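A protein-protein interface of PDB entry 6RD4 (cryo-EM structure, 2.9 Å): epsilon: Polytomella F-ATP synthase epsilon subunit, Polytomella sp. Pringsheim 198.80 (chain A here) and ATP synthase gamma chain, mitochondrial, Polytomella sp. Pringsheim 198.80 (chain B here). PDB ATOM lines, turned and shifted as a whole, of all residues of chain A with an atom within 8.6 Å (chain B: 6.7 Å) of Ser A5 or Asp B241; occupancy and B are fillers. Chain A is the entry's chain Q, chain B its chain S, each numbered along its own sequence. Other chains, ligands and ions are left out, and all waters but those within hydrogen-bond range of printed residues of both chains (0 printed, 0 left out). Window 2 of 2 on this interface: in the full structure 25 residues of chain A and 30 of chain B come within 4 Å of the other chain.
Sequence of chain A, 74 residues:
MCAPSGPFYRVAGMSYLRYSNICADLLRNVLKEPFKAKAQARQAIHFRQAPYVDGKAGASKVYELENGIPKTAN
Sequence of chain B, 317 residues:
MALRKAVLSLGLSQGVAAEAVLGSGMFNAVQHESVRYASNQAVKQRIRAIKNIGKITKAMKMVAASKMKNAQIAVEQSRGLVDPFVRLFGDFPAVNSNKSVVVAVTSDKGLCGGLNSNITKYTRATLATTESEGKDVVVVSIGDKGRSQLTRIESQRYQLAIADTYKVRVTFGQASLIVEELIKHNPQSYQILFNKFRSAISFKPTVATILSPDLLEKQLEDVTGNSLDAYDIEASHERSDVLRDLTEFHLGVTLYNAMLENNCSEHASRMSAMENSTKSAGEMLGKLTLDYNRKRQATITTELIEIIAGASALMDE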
ATOM      1  N   ALA A   3       5.435  -6.263 -11.978  1.00  0.00           N
ATOM      2  CA  ALA A   3       4.479  -7.261 -12.449  1.00  0.00           C
ATOM      3  C   ALA A   3       4.571  -7.605 -13.956  1.00  0.00           C
ATOM      4  O   ALA A   3       4.309  -8.755 -14.312  1.00  0.00           O
ATOM      5  CB  ALA A   3       3.049  -6.834 -12.080  1.00  0.00           C
ATOM      6  N   PRO A   4       4.921  -6.670 -14.848  1.00  0.00           N
ATOM      7  CA  PRO A   4       5.434  -7.099 -16.151  1.00  0.00           C
ATOM      8  C   PRO A   4       6.925  -7.371 -16.063  1.00  0.00           C
ATOM      9  O   PRO A   4       7.614  -6.915 -15.151  1.00  0.00           O
ATOM     10  CB  PRO A   4       5.142  -5.910 -17.078  1.00  0.00           C
ATOM     11  CG  PRO A   4       4.170  -5.073 -16.340  1.00  0.00           C
ATOM     12  CD  PRO A   4       4.573  -5.237 -14.917  1.00  0.00           C
ATOM     13  N   SER A   5       7.414  -8.127 -17.035  1.00  0.00           N
ATOM     14  CA  SER A   5       8.810  -8.538 -17.087  1.00  0.00           C
ATOM     15  C   SER A   5       9.415  -8.037 -18.387  1.00  0.00           C
ATOM     16  O   SER A   5       8.890  -8.320 -19.467  1.00  0.00           O
ATOM     17  CB  SER A   5       8.934 -10.057 -16.979  1.00  0.00           C
ATOM     18  OG  SER A   5       8.348 -10.700 -18.094  1.00  0.00           O
ATOM     19  N   GLY A   6      10.512  -7.301 -18.283  1.00  0.00           N
ATOM     20  CA  GLY A   6      11.176  -6.766 -19.443  1.00  0.00           C
ATOM     21  C   GLY A   6      12.081  -5.605 -19.114  1.00  0.00           C
ATOM     22  O   GLY A   6      12.694  -5.549 -18.045  1.00  0.00           O
ATOM     23  N   PRO A   7      12.176  -4.644 -20.026  1.00  0.00           N
ATOM     24  CA  PRO A   7      13.040  -3.483 -19.787  1.00  0.00           C
ATOM     25  C   PRO A   7      12.503  -2.537 -18.728  1.00  0.00           C
ATOM     26  O   PRO A   7      11.432  -2.770 -18.164  1.00  0.00           O
ATOM     27  CB  PRO A   7      13.107  -2.812 -21.161  1.00  0.00           C
ATOM     28  CG  PRO A   7      12.642  -3.848 -22.126  1.00  0.00           C
ATOM     29  CD  PRO A   7      11.665  -4.673 -21.402  1.00  0.00           C
ATOM     30  N   PHE A   8      13.247  -1.468 -18.449  1.00  0.00           N
ATOM     31  CA  PHE A   8      12.927  -0.626 -17.306  1.00  0.00           C
ATOM     32  C   PHE A   8      11.682   0.207 -17.527  1.00  0.00           C
ATOM     33  O   PHE A   8      11.063   0.646 -16.553  1.00  0.00           O
ATOM     34  CB  PHE A   8      14.104   0.279 -16.954  1.00  0.00           C
ATOM     35  CG  PHE A   8      14.479   1.261 -18.022  1.00  0.00           C
ATOM     36  CD1 PHE A   8      14.021   2.564 -17.974  1.00  0.00           C
ATOM     37  CD2 PHE A   8      15.339   0.898 -19.044  1.00  0.00           C
ATOM     38  CE1 PHE A   8      14.383   3.469 -18.940  1.00  0.00           C
ATOM     39  CE2 PHE A   8      15.703   1.797 -20.011  1.00  0.00           C
ATOM     40  CZ  PHE A   8      15.228   3.085 -19.957  1.00  0.00           C
ATOM     41  N   TYR A   9      11.305   0.443 -18.774  1.00  0.00           N
ATOM     42  CA  TYR A   9      10.039   1.096 -19.052  1.00  0.00           C
ATOM     43  C   TYR A   9       8.888   0.109 -19.003  1.00  0.00           C
ATOM     44  O   TYR A   9       7.800   0.453 -18.545  1.00  0.00           O
ATOM     45  CB  TYR A   9      10.090   1.793 -20.415  1.00  0.00           C
ATOM     46  CG  TYR A   9      10.653   0.963 -21.541  1.00  0.00           C
ATOM     47  CD1 TYR A   9      11.996   1.024 -21.865  1.00  0.00           C
ATOM     48  CD2 TYR A   9       9.835   0.142 -22.298  1.00  0.00           C
ATOM     49  CE1 TYR A   9      12.507   0.278 -22.891  1.00  0.00           C
ATOM     50  CE2 TYR A   9      10.342  -0.609 -23.321  1.00  0.00           C
ATOM     51  CZ  TYR A   9      11.674  -0.537 -23.613  1.00  0.00           C
ATOM     52  OH  TYR A   9      12.177  -1.285 -24.639  1.00  0.00           O
ATOM     53  N   ARG A  10       9.124  -1.127 -19.434  1.00  0.00           N
ATOM     54  CA  ARG A  10       8.036  -2.087 -19.545  1.00  0.00           C
ATOM     55  C   ARG A  10       7.627  -2.637 -18.187  1.00  0.00           C
ATOM     56  O   ARG A  10       6.438  -2.873 -17.955  1.00  0.00           O
ATOM     57  CB  ARG A  10       8.442  -3.215 -20.482  1.00  0.00           C
ATOM     58  CG  ARG A  10       7.323  -4.117 -20.882  1.00  0.00           C
ATOM     59  CD  ARG A  10       6.321  -3.378 -21.726  1.00  0.00           C
ATOM     60  NE  ARG A  10       6.848  -3.040 -23.042  1.00  0.00           N
ATOM     61  CZ  ARG A  10       6.091  -2.629 -24.051  1.00  0.00           C
ATOM     62  NH1 ARG A  10       4.783  -2.524 -23.891  1.00  0.00           N
ATOM     63  NH2 ARG A  10       6.633  -2.343 -25.222  1.00  0.00           N
ATOM     64  N   VAL A  11       8.581  -2.825 -17.272  1.00  0.00           N
ATOM     65  CA  VAL A  11       8.224  -3.254 -15.923  1.00  0.00           C
ATOM     66  C   VAL A  11       7.602  -2.122 -15.119  1.00  0.00           C
ATOM     67  O   VAL A  11       6.909  -2.385 -14.129  1.00  0.00           O
ATOM     68  CB  VAL A  11       9.429  -3.834 -15.157  1.00  0.00           C
ATOM     69  CG1 VAL A  11      10.093  -4.909 -15.965  1.00  0.00           C
ATOM     70  CG2 VAL A  11      10.439  -2.755 -14.806  1.00  0.00           C
ATOM     71  N   ALA A  12       7.805  -0.874 -15.531  1.00  0.00           N
ATOM     72  CA  ALA A  12       7.190   0.271 -14.887  1.00  0.00           C
ATOM     73  C   ALA A  12       5.834   0.614 -15.484  1.00  0.00           C
ATOM     74  O   ALA A  12       5.338   1.721 -15.266  1.00  0.00           O
ATOM     75  CB  ALA A  12       8.118   1.483 -14.965  1.00  0.00           C
ATOM     76  N   GLY A  13       5.239  -0.300 -16.251  1.00  0.00           N
ATOM     77  CA  GLY A  13       3.943  -0.091 -16.862  1.00  0.00           C
ATOM     78  C   GLY A  13       3.958   0.737 -18.127  1.00  0.00           C
ATOM     79  O   GLY A  13       2.954   0.750 -18.849  1.00  0.00           O
ATOM     80  N   TYR A  16       6.493   1.123 -24.921  1.00  0.00           N
ATOM     81  CA  TYR A  16       7.703   1.532 -25.622  1.00  0.00           C
ATOM     82  C   TYR A  16       7.492   2.843 -26.363  1.00  0.00           C
ATOM     83  O   TYR A  16       8.424   3.641 -26.493  1.00  0.00           O
ATOM     84  CB  TYR A  16       8.156   0.442 -26.590  1.00  0.00           C
ATOM     85  CG  TYR A  16       9.325   0.876 -27.426  1.00  0.00           C
ATOM     86  CD1 TYR A  16      10.588   0.950 -26.882  1.00  0.00           C
ATOM     87  CD2 TYR A  16       9.160   1.250 -28.752  1.00  0.00           C
ATOM     88  CE1 TYR A  16      11.652   1.369 -27.629  1.00  0.00           C
ATOM     89  CE2 TYR A  16      10.217   1.683 -29.495  1.00  0.00           C
ATOM     90  CZ  TYR A  16      11.460   1.731 -28.932  1.00  0.00           C
ATOM     91  OH  TYR A  16      12.525   2.144 -29.678  1.00  0.00           O
ATOM     92  N   ALA B 235      18.700  -7.107 -28.315  1.00  0.00           N
ATOM     93  CA  ALA B 235      17.941  -6.326 -27.357  1.00  0.00           C
ATOM     94  C   ALA B 235      18.469  -6.528 -25.950  1.00  0.00           C
ATOM     95  O   ALA B 235      19.381  -7.315 -25.701  1.00  0.00           O
ATOM     96  CB  ALA B 235      16.466  -6.695 -27.407  1.00  0.00           C
ATOM     97  N   HIS B 237      16.280  -7.523 -23.346  1.00  0.00           N
ATOM     98  CA  HIS B 237      15.534  -8.686 -22.932  1.00  0.00           C
ATOM     99  C   HIS B 237      15.212  -9.571 -24.135  1.00  0.00           C
ATOM    100  O   HIS B 237      15.901  -9.515 -25.157  1.00  0.00           O
ATOM    101  CB  HIS B 237      14.324  -8.218 -22.154  1.00  0.00           C
ATOM    102  CG  HIS B 237      14.682  -7.603 -20.844  1.00  0.00           C
ATOM    103  ND1 HIS B 237      15.253  -6.354 -20.742  1.00  0.00           N
ATOM    104  CD2 HIS B 237      14.585  -8.076 -19.581  1.00  0.00           C
ATOM    105  CE1 HIS B 237      15.476  -6.077 -19.471  1.00  0.00           C
ATOM    106  NE2 HIS B 237      15.076  -7.103 -18.746  1.00  0.00           N
ATOM    107  N   GLU B 238      14.217 -10.436 -23.980  1.00  0.00           N
ATOM    108  CA  GLU B 238      13.972 -11.528 -24.909  1.00  0.00           C
ATOM    109  C   GLU B 238      13.474 -11.028 -26.259  1.00  0.00           C
ATOM    110  O   GLU B 238      13.096  -9.869 -26.432  1.00  0.00           O
ATOM    111  CB  GLU B 238      12.945 -12.498 -24.338  1.00  0.00           C
ATOM    112  CG  GLU B 238      13.161 -12.877 -22.890  1.00  0.00           C
ATOM    113  CD  GLU B 238      14.596 -13.228 -22.589  1.00  0.00           C
ATOM    114  OE1 GLU B 238      15.187 -12.570 -21.709  1.00  0.00           O
ATOM    115  OE2 GLU B 238      15.134 -14.140 -23.250  1.00  0.00           O
ATOM    116  N   ARG B 239      13.472 -11.948 -27.226  1.00  0.00           N
ATOM    117  CA  ARG B 239      12.920 -11.656 -28.541  1.00  0.00           C
ATOM    118  C   ARG B 239      11.421 -11.430 -28.468  1.00  0.00           C
ATOM    119  O   ARG B 239      10.881 -10.558 -29.155  1.00  0.00           O
ATOM    120  CB  ARG B 239      13.223 -12.797 -29.501  1.00  0.00           C
ATOM    121  CG  ARG B 239      12.796 -12.515 -30.909  1.00  0.00           C
ATOM    122  CD  ARG B 239      13.123 -13.650 -31.810  1.00  0.00           C
ATOM    123  NE  ARG B 239      12.250 -14.781 -31.552  1.00  0.00           N
ATOM    124  CZ  ARG B 239      12.111 -15.803 -32.381  1.00  0.00           C
ATOM    125  NH1 ARG B 239      12.795 -15.825 -33.514  1.00  0.00           N
ATOM    126  NH2 ARG B 239      11.295 -16.797 -32.076  1.00  0.00           N
ATOM    127  N   SER B 240      10.732 -12.182 -27.612  1.00  0.00           N
ATOM    128  CA  SER B 240       9.311 -11.961 -27.384  1.00  0.00           C
ATOM    129  C   SER B 240       9.037 -10.640 -26.690  1.00  0.00           C
ATOM    130  O   SER B 240       7.892 -10.187 -26.672  1.00  0.00           O
ATOM    131  CB  SER B 240       8.734 -13.100 -26.548  1.00  0.00           C
ATOM    132  OG  SER B 240       9.261 -13.065 -25.234  1.00  0.00           O
ATOM    133  N   ASP B 241      10.056 -10.031 -26.105  1.00  0.00           N
ATOM    134  CA  ASP B 241       9.947  -8.768 -25.404  1.00  0.00           C
ATOM    135  C   ASP B 241      10.323  -7.598 -26.298  1.00  0.00           C
ATOM    136  O   ASP B 241       9.766  -6.505 -26.156  1.00  0.00           O
ATOM    137  CB  ASP B 241      10.854  -8.817 -24.186  1.00  0.00           C
ATOM    138  CG  ASP B 241      10.358  -7.978 -23.073  1.00  0.00           C
ATOM    139  OD1 ASP B 241       9.998  -6.805 -23.288  1.00  0.00           O
ATOM    140  OD2 ASP B 241      10.287  -8.534 -21.965  1.00  0.00           O
ATOM    141  N   VAL B 242      11.261  -7.805 -27.223  1.00  0.00           N
ATOM    142  CA  VAL B 242      11.587  -6.740 -28.156  1.00  0.00           C
ATOM    143  C   VAL B 242      10.494  -6.625 -29.204  1.00  0.00           C
ATOM    144  O   VAL B 242      10.193  -5.522 -29.658  1.00  0.00           O
ATOM    145  CB  VAL B 242      12.991  -6.942 -28.773  1.00  0.00           C
ATOM    146  CG1 VAL B 242      13.053  -8.085 -29.743  1.00  0.00           C
ATOM    147  CG2 VAL B 242      13.452  -5.719 -29.461  1.00  0.00           C
ATOM    148  N   LEU B 243       9.819  -7.731 -29.541  1.00  0.00           N
ATOM    149  CA  LEU B 243       8.710  -7.670 -30.485  1.00  0.00           C
ATOM    150  C   LEU B 243       7.495  -7.004 -29.873  1.00  0.00           C
ATOM    151  O   LEU B 243       6.657  -6.469 -30.600  1.00  0.00           O
ATOM    152  CB  LEU B 243       8.344  -9.065 -30.971  1.00  0.00           C
ATOM    153  CG  LEU B 243       8.802  -9.459 -32.364  1.00  0.00           C
ATOM    154  CD1 LEU B 243      10.289  -9.557 -32.430  1.00  0.00           C
ATOM    155  CD2 LEU B 243       8.193 -10.784 -32.715  1.00  0.00           C
ATOM    156  N   ARG B 244       7.375  -7.043 -28.552  1.00  0.00           N
ATOM    157  CA  ARG B 244       6.388  -6.218 -27.879  1.00  0.00           C
ATOM    158  C   ARG B 244       6.722  -4.743 -28.044  1.00  0.00           C
ATOM    159  O   ARG B 244       5.828  -3.923 -28.252  1.00  0.00           O
ATOM    160  CB  ARG B 244       6.310  -6.616 -26.408  1.00  0.00           C
ATOM    161  CG  ARG B 244       5.493  -5.711 -25.528  1.00  0.00           C
ATOM    162  CD  ARG B 244       4.041  -5.762 -25.893  1.00  0.00           C
ATOM    163  NE  ARG B 244       3.440  -7.042 -25.551  1.00  0.00           N
ATOM    164  CZ  ARG B 244       2.162  -7.336 -25.749  1.00  0.00           C
ATOM    165  NH1 ARG B 244       1.695  -8.532 -25.411  1.00  0.00           N
ATOM    166  NH2 ARG B 244       1.352  -6.440 -26.298  1.00  0.00           N
ATOM    167  N   ASP B 245       8.004  -4.388 -27.993  1.00  0.00           N
ATOM    168  CA  ASP B 245       8.390  -3.001 -28.221  1.00  0.00           C
ATOM    169  C   ASP B 245       8.260  -2.629 -29.688  1.00  0.00           C
ATOM    170  O   ASP B 245       7.982  -1.475 -30.022  1.00  0.00           O
ATOM    171  CB  ASP B 245       9.826  -2.764 -27.760  1.00  0.00           C
ATOM    172  CG  ASP B 245       9.998  -2.883 -26.260  1.00  0.00           C
ATOM    173  OD1 ASP B 245       9.028  -2.643 -25.516  1.00  0.00           O
ATOM    174  OD2 ASP B 245      11.120  -3.203 -25.823  1.00  0.00           O
ATOM    175  N   LEU B 246       8.431  -3.601 -30.574  1.00  0.00           N
ATOM    176  CA  LEU B 246       8.642  -3.334 -31.988  1.00  0.00           C
ATOM    177  C   LEU B 246       7.335  -3.216 -32.751  1.00  0.00           C
ATOM    178  O   LEU B 246       7.291  -2.557 -33.790  1.00  0.00           O
ATOM    179  CB  LEU B 246       9.508  -4.437 -32.583  1.00  0.00           C
ATOM    180  CG  LEU B 246      10.123  -4.349 -33.963  1.00  0.00           C
ATOM    181  CD1 LEU B 246      10.791  -3.059 -34.094  1.00  0.00           C
ATOM    182  CD2 LEU B 246      11.136  -5.435 -34.105  1.00  0.00           C
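Of the 12 printed residues of chain A, 6 touch a printed residue of chain B.
Among the printed residues, 9 pairs touch across the chains.
The backbone carbonyl oxygen (O) of Gly A6 sits at hydrogen-bond distance from a ring nitrogen (NE2) of His B237 (2.9 Å).
NH2 of Arg A10 lies within salt-bridge range of OD1 of Asp B245, 2.4 Å away.
The side-chain carboxylate of Asp B241 lies close to the backbone carbonyl oxygen of Ser A5 (2.9 Å).
The side-chain hydroxyl (OH) of Tyr A9 is in hydrogen-bond range of the side-chain carboxylate (OD2) of Asp B245 (2.5 Å).
No residue of chain A comes within 4 Å of Ser B240.
Printed residues of chain A within 4 Å of Arg B244: Arg A10.
Of the printed residues of chain B, Pro A7 touches His B237 and Asp B241.
Of the printed residues of chain A, Asp B245 touches Tyr A9 (2.5 Å), Arg A10 (2.4 Å) and Tyr A16 (3.2 Å).
Printed residues of chain A within 4 Å of His B237: Gly A6 (2.9 Å) and Pro A7 (3.6 Å).
Glu B238 touches none of the printed residues of chain A.
The nearest residue of chain A that does not touch Asp B241 is Arg A10 (4.5 Å).
The nearest printed residue of chain A that does not touch Asp B245 is Pro A7 (4.05 Å).
Asp B241 touches Gly A6.
His B237 touches Pro A7 (CE1 to CA, 3.6 Å).
Asp B241 touches Pro A7 (OD1 to CD, 3.3 Å).
CG of Arg B244 touches CZ of Arg A10, 3.5 Å away.
Asp B245 touches Tyr A16.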
